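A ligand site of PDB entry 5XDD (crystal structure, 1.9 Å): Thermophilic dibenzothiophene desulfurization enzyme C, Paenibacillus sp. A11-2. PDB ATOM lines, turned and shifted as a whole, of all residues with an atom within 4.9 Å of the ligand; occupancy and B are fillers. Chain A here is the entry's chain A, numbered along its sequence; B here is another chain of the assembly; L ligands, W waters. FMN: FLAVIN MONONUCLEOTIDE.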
ATOM      1  N   HIS A  89     -24.034  22.733  17.357  1.00  0.00           N
ATOM      2  CA  HIS A  89     -23.999  21.800  16.250  1.00  0.00           C
ATOM      3  C   HIS A  89     -23.815  20.347  16.725  1.00  0.00           C
ATOM      4  O   HIS A  89     -24.516  19.446  16.249  1.00  0.00           O
ATOM      5  CB  HIS A  89     -22.879  22.209  15.326  1.00  0.00           C
ATOM      6  CG  HIS A  89     -22.593  21.220  14.260  1.00  0.00           C
ATOM      7  ND1 HIS A  89     -23.171  21.288  13.011  1.00  0.00           N
ATOM      8  CD2 HIS A  89     -21.760  20.145  14.233  1.00  0.00           C
ATOM      9  CE1 HIS A  89     -22.711  20.294  12.269  1.00  0.00           C
ATOM     10  NE2 HIS A  89     -21.854  19.594  12.987  1.00  0.00           N
ATOM     11  N   TYR A  93     -26.586  17.586  16.152  1.00  0.00           N
ATOM     12  CA  TYR A  93     -26.303  16.429  15.318  1.00  0.00           C
ATOM     13  C   TYR A  93     -26.442  15.117  16.098  1.00  0.00           C
ATOM     14  O   TYR A  93     -26.843  14.089  15.533  1.00  0.00           O
ATOM     15  CB  TYR A  93     -24.919  16.529  14.710  1.00  0.00           C
ATOM     16  CG  TYR A  93     -24.960  16.449  13.187  1.00  0.00           C
ATOM     17  CD1 TYR A  93     -25.496  15.319  12.548  1.00  0.00           C
ATOM     18  CD2 TYR A  93     -24.489  17.488  12.395  1.00  0.00           C
ATOM     19  CE1 TYR A  93     -25.562  15.237  11.147  1.00  0.00           C
ATOM     20  CE2 TYR A  93     -24.533  17.420  11.003  1.00  0.00           C
ATOM     21  CZ  TYR A  93     -25.075  16.291  10.377  1.00  0.00           C
ATOM     22  OH  TYR A  93     -25.129  16.232   8.995  1.00  0.00           O
ATOM     23  N   ASN A 126     -21.284  10.768  13.761  1.00  0.00           N
ATOM     24  CA  ASN A 126     -21.644  10.086  12.537  1.00  0.00           C
ATOM     25  C   ASN A 126     -20.537  10.176  11.495  1.00  0.00           C
ATOM     26  O   ASN A 126     -19.717  11.096  11.487  1.00  0.00           O
ATOM     27  CB  ASN A 126     -22.930  10.630  11.922  1.00  0.00           C
ATOM     28  CG  ASN A 126     -22.691  11.888  11.136  1.00  0.00           C
ATOM     29  OD1 ASN A 126     -22.553  11.844   9.907  1.00  0.00           O
ATOM     30  ND2 ASN A 126     -22.618  13.016  11.833  1.00  0.00           N
ATOM     31  N   SER A 128     -20.885   9.693   7.426  1.00  0.00           N
ATOM     32  CA  SER A 128     -21.890   9.527   6.371  1.00  0.00           C
ATOM     33  C   SER A 128     -21.398  10.040   5.033  1.00  0.00           C
ATOM     34  O   SER A 128     -21.319   9.292   4.047  1.00  0.00           O
ATOM     35  CB  SER A 128     -23.173  10.291   6.732  1.00  0.00           C
ATOM     36  OG  SER A 128     -23.561  10.051   8.068  1.00  0.00           O
ATOM     37  N   SER A 129     -21.063  11.325   4.986  1.00  0.00           N
ATOM     38  CA  SER A 129     -20.649  11.976   3.746  1.00  0.00           C
ATOM     39  C   SER A 129     -19.249  11.530   3.348  1.00  0.00           C
ATOM     40  O   SER A 129     -18.476  11.009   4.160  1.00  0.00           O
ATOM     41  CB  SER A 129     -20.666  13.507   3.900  1.00  0.00           C
ATOM     42  OG  SER A 129     -21.995  14.013   3.969  1.00  0.00           O
ATOM     43  N   VAL A 135     -21.552  14.934  -4.577  1.00  0.00           N
ATOM     44  CA  VAL A 135     -22.064  14.726  -3.230  1.00  0.00           C
ATOM     45  C   VAL A 135     -22.727  13.361  -3.075  1.00  0.00           C
ATOM     46  O   VAL A 135     -22.720  12.769  -1.984  1.00  0.00           O
ATOM     47  CB  VAL A 135     -23.017  15.881  -2.864  1.00  0.00           C
ATOM     48  CG1 VAL A 135     -24.442  15.638  -3.424  1.00  0.00           C
ATOM     49  CG2 VAL A 135     -23.021  16.113  -1.338  1.00  0.00           C
ATOM     50  N   PHE A 158     -16.287  14.950   6.684  1.00  0.00           N
ATOM     51  CA  PHE A 158     -17.223  15.767   7.462  1.00  0.00           C
ATOM     52  C   PHE A 158     -17.942  14.943   8.528  1.00  0.00           C
ATOM     53  O   PHE A 158     -19.167  14.960   8.644  1.00  0.00           O
ATOM     54  CB  PHE A 158     -18.274  16.441   6.553  1.00  0.00           C
ATOM     55  CG  PHE A 158     -17.739  17.548   5.678  1.00  0.00           C
ATOM     56  CD1 PHE A 158     -17.651  18.851   6.148  1.00  0.00           C
ATOM     57  CD2 PHE A 158     -17.391  17.287   4.368  1.00  0.00           C
ATOM     58  CE1 PHE A 158     -17.188  19.879   5.328  1.00  0.00           C
ATOM     59  CE2 PHE A 158     -16.915  18.310   3.547  1.00  0.00           C
ATOM     60  CZ  PHE A 158     -16.820  19.608   4.028  1.00  0.00           C
ATOM     61  N   CYS A 159     -17.156  14.216   9.324  1.00  0.00           N
ATOM     62  CA  CYS A 159     -17.720  13.304  10.326  1.00  0.00           C
ATOM     63  C   CYS A 159     -17.963  14.027  11.642  1.00  0.00           C
ATOM     64  O   CYS A 159     -17.265  13.833  12.639  1.00  0.00           O
ATOM     65  CB  CYS A 159     -16.797  12.110  10.494  1.00  0.00           C
ATOM     66  SG  CYS A 159     -16.629  11.239   8.993  1.00  0.00           S
ATOM     67  N   SER A 160     -18.990  14.857  11.651  1.00  0.00           N
ATOM     68  CA  SER A 160     -19.227  15.718  12.791  1.00  0.00           C
ATOM     69  C   SER A 160     -19.334  14.923  14.071  1.00  0.00           C
ATOM     70  O   SER A 160     -20.022  13.881  14.139  1.00  0.00           O
ATOM     71  CB  SER A 160     -20.491  16.555  12.596  1.00  0.00           C
ATOM     72  OG  SER A 160     -20.261  17.560  11.630  1.00  0.00           O
ATOM     73  N   TRP A 202      -9.725  18.547  11.019  1.00  0.00           N
ATOM     74  CA  TRP A 202     -10.729  19.606  10.889  1.00  0.00           C
ATOM     75  C   TRP A 202     -10.077  20.942  11.268  1.00  0.00           C
ATOM     76  O   TRP A 202      -9.653  21.126  12.419  1.00  0.00           O
ATOM     77  CB  TRP A 202     -11.924  19.302  11.789  1.00  0.00           C
ATOM     78  CG  TRP A 202     -13.072  20.292  11.719  1.00  0.00           C
ATOM     79  CD1 TRP A 202     -13.573  21.031  12.742  1.00  0.00           C
ATOM     80  CD2 TRP A 202     -13.864  20.622  10.555  1.00  0.00           C
ATOM     81  NE1 TRP A 202     -14.610  21.834  12.303  1.00  0.00           N
ATOM     82  CE2 TRP A 202     -14.809  21.596  10.963  1.00  0.00           C
ATOM     83  CE3 TRP A 202     -13.852  20.204   9.220  1.00  0.00           C
ATOM     84  CZ2 TRP A 202     -15.757  22.137  10.092  1.00  0.00           C
ATOM     85  CZ3 TRP A 202     -14.785  20.748   8.332  1.00  0.00           C
ATOM     86  CH2 TRP A 202     -15.724  21.726   8.782  1.00  0.00           C
ATOM     87  N   MET A 207     -17.242  26.939  12.881  1.00  0.00           N
ATOM     88  CA  MET A 207     -17.614  25.633  13.411  1.00  0.00           C
ATOM     89  C   MET A 207     -16.347  24.849  13.785  1.00  0.00           C
ATOM     90  O   MET A 207     -16.221  23.648  13.536  1.00  0.00           O
ATOM     91  CB  MET A 207     -18.523  24.875  12.426  1.00  0.00           C
ATOM     92  CG  MET A 207     -19.905  25.558  12.276  1.00  0.00           C
ATOM     93  SD  MET A 207     -20.922  25.353  13.770  1.00  0.00           S
ATOM     94  CE  MET A 207     -22.316  26.333  13.336  1.00  0.00           C
ATOM     95  N   THR A 210     -16.349  21.377  15.993  1.00  0.00           N
ATOM     96  CA  THR A 210     -17.286  20.305  15.672  1.00  0.00           C
ATOM     97  C   THR A 210     -16.607  18.987  15.311  1.00  0.00           C
ATOM     98  O   THR A 210     -17.303  17.962  15.170  1.00  0.00           O
ATOM     99  CB  THR A 210     -18.207  20.701  14.484  1.00  0.00           C
ATOM    100  OG1 THR A 210     -17.425  20.957  13.307  1.00  0.00           O
ATOM    101  CG2 THR A 210     -19.013  21.924  14.822  1.00  0.00           C
ATOM    102  N   SER A 212     -15.327  17.882  12.558  1.00  0.00           N
ATOM    103  CA  SER A 212     -15.953  17.377  11.335  1.00  0.00           C
ATOM    104  C   SER A 212     -14.909  16.973  10.301  1.00  0.00           C
ATOM    105  O   SER A 212     -15.008  17.279   9.102  1.00  0.00           O
ATOM    106  CB  SER A 212     -16.922  18.420  10.761  1.00  0.00           C
ATOM    107  OG  SER A 212     -17.915  18.762  11.728  1.00  0.00           O
ATOM    108  N   THR A 384     -19.874  29.194   7.561  1.00  0.00           N
ATOM    109  CA  THR A 384     -19.407  27.826   7.329  1.00  0.00           C
ATOM    110  C   THR A 384     -20.588  26.880   7.240  1.00  0.00           C
ATOM    111  O   THR A 384     -20.734  26.144   6.258  1.00  0.00           O
ATOM    112  CB  THR A 384     -18.439  27.398   8.438  1.00  0.00           C
ATOM    113  OG1 THR A 384     -17.310  28.276   8.459  1.00  0.00           O
ATOM    114  CG2 THR A 384     -17.942  25.970   8.224  1.00  0.00           C
ATOM    115  N   HIS A 385     -21.465  26.895   8.236  1.00  0.00           N
ATOM    116  CA  HIS A 385     -22.461  25.840   8.332  1.00  0.00           C
ATOM    117  C   HIS A 385     -23.549  25.964   7.265  1.00  0.00           C
ATOM    118  O   HIS A 385     -24.056  24.938   6.775  1.00  0.00           O
ATOM    119  CB  HIS A 385     -23.103  25.837   9.696  1.00  0.00           C
ATOM    120  CG  HIS A 385     -23.812  24.567   9.981  1.00  0.00           C
ATOM    121  ND1 HIS A 385     -24.925  24.188   9.275  1.00  0.00           N
ATOM    122  CD2 HIS A 385     -23.536  23.556  10.824  1.00  0.00           C
ATOM    123  CE1 HIS A 385     -25.313  22.990   9.684  1.00  0.00           C
ATOM    124  NE2 HIS A 385     -24.490  22.592  10.631  1.00  0.00           N
ATOM    125  N   LEU A 387     -23.470  26.485   4.328  1.00  0.00           N
ATOM    126  CA  LEU A 387     -23.078  25.839   3.094  1.00  0.00           C
ATOM    127  C   LEU A 387     -23.242  24.317   3.137  1.00  0.00           C
ATOM    128  O   LEU A 387     -22.870  23.644   2.168  1.00  0.00           O
ATOM    129  CB  LEU A 387     -21.613  26.190   2.771  1.00  0.00           C
ATOM    130  CG  LEU A 387     -21.259  27.690   2.716  1.00  0.00           C
ATOM    131  CD1 LEU A 387     -19.763  27.919   2.685  1.00  0.00           C
ATOM    132  CD2 LEU A 387     -21.918  28.357   1.514  1.00  0.00           C
ATOM    133  N   HIS A 388     -23.734  23.775   4.250  1.00  0.00           N
ATOM    134  CA  HIS A 388     -23.892  22.326   4.418  1.00  0.00           C
ATOM    135  C   HIS A 388     -24.559  21.718   3.195  1.00  0.00           C
ATOM    136  O   HIS A 388     -24.083  20.735   2.624  1.00  0.00           O
ATOM    137  CB  HIS A 388     -24.710  22.053   5.680  1.00  0.00           C
ATOM    138  CG  HIS A 388     -24.923  20.600   5.978  1.00  0.00           C
ATOM    139  ND1 HIS A 388     -25.874  19.834   5.325  1.00  0.00           N
ATOM    140  CD2 HIS A 388     -24.327  19.772   6.884  1.00  0.00           C
ATOM    141  CE1 HIS A 388     -25.835  18.607   5.801  1.00  0.00           C
ATOM    142  NE2 HIS A 388     -24.911  18.536   6.735  1.00  0.00           N
ATOM    143  N   ASP A 389     -25.674  22.303   2.783  1.00  0.00           N
ATOM    144  CA  ASP A 389     -26.196  22.042   1.458  1.00  0.00           C
ATOM    145  C   ASP A 389     -26.685  23.364   0.870  1.00  0.00           C
ATOM    146  O   ASP A 389     -27.063  24.280   1.599  1.00  0.00           O
ATOM    147  CB  ASP A 389     -27.315  20.978   1.458  1.00  0.00           C
ATOM    148  CG  ASP A 389     -28.418  21.269   2.446  1.00  0.00           C
ATOM    149  OD1 ASP A 389     -28.261  20.884   3.629  1.00  0.00           O
ATOM    150  OD2 ASP A 389     -29.422  21.864   2.031  1.00  0.00           O
ATOM    151  N   TYR A 413     -31.000  14.665   1.679  1.00  0.00           N
ATOM    152  CA  TYR A 413     -30.926  16.114   1.582  1.00  0.00           C
ATOM    153  C   TYR A 413     -32.273  16.790   1.425  1.00  0.00           C
ATOM    154  O   TYR A 413     -32.366  17.996   1.674  1.00  0.00           O
ATOM    155  CB  TYR A 413     -30.038  16.516   0.402  1.00  0.00           C
ATOM    156  CG  TYR A 413     -28.557  16.426   0.706  1.00  0.00           C
ATOM    157  CD1 TYR A 413     -27.960  17.312   1.602  1.00  0.00           C
ATOM    158  CD2 TYR A 413     -27.768  15.438   0.124  1.00  0.00           C
ATOM    159  CE1 TYR A 413     -26.614  17.230   1.897  1.00  0.00           C
ATOM    160  CE2 TYR A 413     -26.410  15.351   0.417  1.00  0.00           C
ATOM    161  CZ  TYR A 413     -25.837  16.256   1.302  1.00  0.00           C
ATOM    162  OH  TYR A 413     -24.493  16.203   1.618  1.00  0.00           O
ATOM    163  N   ARG B 279     -17.338  21.495  -6.405  1.00  0.00           N
ATOM    164  CA  ARG B 279     -17.998  20.336  -7.006  1.00  0.00           C
ATOM    165  C   ARG B 279     -19.390  20.717  -7.508  1.00  0.00           C
ATOM    166  O   ARG B 279     -20.067  21.559  -6.907  1.00  0.00           O
ATOM    167  CB  ARG B 279     -18.129  19.199  -5.989  1.00  0.00           C
ATOM    168  CG  ARG B 279     -16.862  18.382  -5.769  1.00  0.00           C
ATOM    169  CD  ARG B 279     -16.180  18.784  -4.484  1.00  0.00           C
ATOM    170  NE  ARG B 279     -15.321  17.723  -3.937  1.00  0.00           N
ATOM    171  CZ  ARG B 279     -14.061  17.490  -4.308  1.00  0.00           C
ATOM    172  NH1 ARG B 279     -13.473  18.235  -5.245  1.00  0.00           N
ATOM    173  NH2 ARG B 279     -13.373  16.510  -3.735  1.00  0.00           N
ATOM    174  N   MET B 363     -19.075  29.019  -4.114  1.00  0.00           N
ATOM    175  CA  MET B 363     -17.880  28.181  -4.045  1.00  0.00           C
ATOM    176  C   MET B 363     -18.137  26.835  -3.374  1.00  0.00           C
ATOM    177  O   MET B 363     -17.591  25.813  -3.802  1.00  0.00           O
ATOM    178  CB  MET B 363     -16.760  28.924  -3.296  1.00  0.00           C
ATOM    179  CG  MET B 363     -16.215  30.100  -4.068  1.00  0.00           C
ATOM    180  SD  MET B 363     -14.779  30.882  -3.261  1.00  0.00           S
ATOM    181  CE  MET B 363     -15.574  31.718  -1.933  1.00  0.00           C
ATOM    182  N   GLY B 364     -18.969  26.801  -2.347  1.00  0.00           N
ATOM    183  CA  GLY B 364     -19.331  25.575  -1.675  1.00  0.00           C
ATOM    184  C   GLY B 364     -18.686  25.448  -0.307  1.00  0.00           C
ATOM    185  O   GLY B 364     -17.766  26.181   0.075  1.00  0.00           O
ATOM    186  N   ALA B 365     -19.187  24.460   0.438  1.00  0.00           N
ATOM    187  CA  ALA B 365     -18.746  24.265   1.816  1.00  0.00           C
ATOM    188  C   ALA B 365     -17.236  24.128   1.940  1.00  0.00           C
ATOM    189  O   ALA B 365     -16.665  24.585   2.928  1.00  0.00           O
ATOM    190  CB  ALA B 365     -19.431  23.029   2.384  1.00  0.00           C
ATOM    191  N   ARG B 366     -16.557  23.528   0.962  1.00  0.00           N
ATOM    192  CA  ARG B 366     -15.125  23.291   1.164  1.00  0.00           C
ATOM    193  C   ARG B 366     -14.318  24.572   1.150  1.00  0.00           C
ATOM    194  O   ARG B 366     -13.200  24.602   1.678  1.00  0.00           O
ATOM    195  CB  ARG B 366     -14.606  22.300   0.121  1.00  0.00           C
ATOM    196  CG  ARG B 366     -14.943  20.843   0.502  1.00  0.00           C
ATOM    197  CD  ARG B 366     -15.386  20.000  -0.684  1.00  0.00           C
ATOM    198  NE  ARG B 366     -14.387  19.969  -1.755  1.00  0.00           N
ATOM    199  CZ  ARG B 366     -14.415  20.736  -2.847  1.00  0.00           C
ATOM    200  NH1 ARG B 366     -15.424  21.581  -3.064  1.00  0.00           N
ATOM    201  NH2 ARG B 366     -13.445  20.621  -3.748  1.00  0.00           N
HETATM  202  N1  FMN L   1     -22.136  15.668   6.261  1.00  0.00           N
HETATM  203  C2  FMN L   1     -22.534  14.540   6.936  1.00  0.00           C
HETATM  204  O2  FMN L   1     -22.871  13.543   6.282  1.00  0.00           O
HETATM  205  N3  FMN L   1     -22.537  14.497   8.310  1.00  0.00           N
HETATM  206  C4  FMN L   1     -22.151  15.617   9.020  1.00  0.00           C
HETATM  207  O4  FMN L   1     -22.164  15.567  10.265  1.00  0.00           O
HETATM  208  C4A FMN L   1     -21.763  16.774   8.347  1.00  0.00           C
HETATM  209  N5  FMN L   1     -21.364  17.888   9.056  1.00  0.00           N
HETATM  210  C5A FMN L   1     -20.972  19.037   8.386  1.00  0.00           C
HETATM  211  C6  FMN L   1     -20.582  20.156   9.129  1.00  0.00           C
HETATM  212  C7  FMN L   1     -20.187  21.325   8.483  1.00  0.00           C
HETATM  213  C7M FMN L   1     -19.787  22.492   9.338  1.00  0.00           C
HETATM  214  C8  FMN L   1     -20.174  21.363   7.074  1.00  0.00           C
HETATM  215  C8M FMN L   1     -19.762  22.588   6.309  1.00  0.00           C
HETATM  216  C9  FMN L   1     -20.557  20.239   6.342  1.00  0.00           C
HETATM  217  C9A FMN L   1     -20.963  19.063   6.984  1.00  0.00           C
HETATM  218  N10 FMN L   1     -21.375  17.946   6.246  1.00  0.00           N
HETATM  219  C10 FMN L   1     -21.755  16.800   6.945  1.00  0.00           C
HETATM  220  C1' FMN L   1     -21.298  17.912   4.714  1.00  0.00           C
HETATM  221  C2' FMN L   1     -22.211  18.671   3.772  1.00  0.00           C
HETATM  222  O2' FMN L   1     -23.516  18.126   3.850  1.00  0.00           O
HETATM  223  C3' FMN L   1     -21.678  18.541   2.339  1.00  0.00           C
HETATM  224  O3' FMN L   1     -21.034  17.292   2.162  1.00  0.00           O
HETATM  225  C4' FMN L   1     -20.702  19.651   1.943  1.00  0.00           C
HETATM  226  O4' FMN L   1     -21.344  20.892   2.169  1.00  0.00           O
HETATM  227  C5' FMN L   1     -20.240  19.544   0.477  1.00  0.00           C
HETATM  228  O5' FMN L   1     -19.220  20.482   0.131  1.00  0.00           O
HETATM  229  P   FMN L   1     -19.174  21.300  -1.287  1.00  0.00           P
HETATM  230  O1P FMN L   1     -20.366  22.269  -1.267  1.00  0.00           O
HETATM  231  O2P FMN L   1     -17.870  22.055  -1.445  1.00  0.00           O
HETATM  232  O3P FMN L   1     -19.248  20.341  -2.452  1.00  0.00           O
HETATM  233  O   HOH W   1     -23.526  19.592  -0.464  1.00  0.00           O
HETATM  234  O   HOH W   2     -20.012  12.539   7.572  1.00  0.00           O
HETATM  235  O   HOH W   3     -16.479  24.025  -2.223  1.00  0.00           O
HETATM  236  O   HOH W   4     -21.733  19.759  -2.938  1.00  0.00           O
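The backbone NH (N) of Ser 129 is in hydrogen-bond range of an oxygen (O2) of the ligand, 3.1 Å away. OG of Ser 129 sits at hydrogen-bond distance from O2 of the ligand, at 2.5 Å. O of His 388 lies within hydrogen-bond range of O4' of the ligand (2.8 Å). A ring nitrogen (NE2) of His 388 sits close to an oxygen (O2') of the ligand, 3.2 Å away. The side-chain hydroxyl (OG) of Ser 160 lies within hydrogen-bond range of a nitrogen (N5) of the ligand (2.8 Å). An oxygen (O1P) of the ligand sits at hydrogen-bond distance from the backbone NH (N) of Ala 365 of chain B. N of Arg 366 of chain B lies within hydrogen-bond range of O2P of the ligand, at 3.1 Å. An oxygen (O2P) of the ligand lies within salt-bridge range of the guanidinium group of Arg 366 of chain B. N3 of the ligand lies close to OH of Tyr 93, at 3.2 Å. An oxygen (O4) of the ligand is in hydrogen-bond range of the side-chain amide nitrogen of Asn 126, 3.0 Å away. The backbone carbonyl oxygen (O) of Phe 158 sits close to a nitrogen (N3) of the ligand (3.4 Å). O2' of the ligand sits at hydrogen-bond distance from OH of Tyr 413, at 3.1 Å. O4' of the ligand is in hydrogen-bond range of O of Leu 387, 3.1 Å away.
The side-chain hydroxyl of Tyr 93 sits at hydrogen-bond distance from a ring nitrogen (NE2) of His 388 (3.2 Å). A ring nitrogen (ND1) of His 388 is in hydrogen-bond range of the side-chain carboxylate (OD1) of Asp 389 (3.1 Å). The backbone carbonyl oxygen of Ser 160 sits at hydrogen-bond distance from the backbone NH of Asn 126. The side-chain hydroxyl (OG) of Ser 160 sits at hydrogen-bond distance from a ring nitrogen (NE2) of His 89 (2.9 Å). OG of Ser 160 lies within hydrogen-bond range of OG of Ser 212 (2.6 Å). The side-chain amide oxygen (OD1) of Asn 126 lies within hydrogen-bond range of the side-chain hydroxyl (OG) of Ser 128 (2.8 Å). A ring nitrogen (ND1) of His 89 lies within hydrogen-bond range of a ring nitrogen (NE2) of His 385 (3.0 Å). The side-chain hydroxyl (OG) of Ser 212 sits at hydrogen-bond distance from the side-chain hydroxyl (OG1) of Thr 210.
Water W3 lies within hydrogen-bond range of O2P of the ligand (2.5 Å), O of Met 363 of chain B (2.6 Å), NH1 of Arg 366 of chain B (2.8 Å) and O of Gly 364 of chain B (3.4 Å).
CE1 of His 89 touches C6 of the ligand (3.8 Å). CB of Ser 128 touches O2 of the ligand, at 3.3 Å. Ser 212 touches the ligand. Thr 384 touches the ligand (O to C8M, 3.7 Å). Arg 279 of chain B touches the ligand. Gly 364 of chain B touches the ligand (CA to O1P, 3.5 Å). Within 4 Å of the ligand: His 89, Tyr 93, Asn 126, Ser 128, Ser 129, Phe 158, Ser 160, Ser 212, Thr 384, Leu 387, His 388, Tyr 413, Arg 279 of chain B, Gly 364 of chain B, Ala 365 of chain B and Arg 366 of chain B. The nearest printed residue that does not touch the ligand is Met 207 (4.1 Å).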
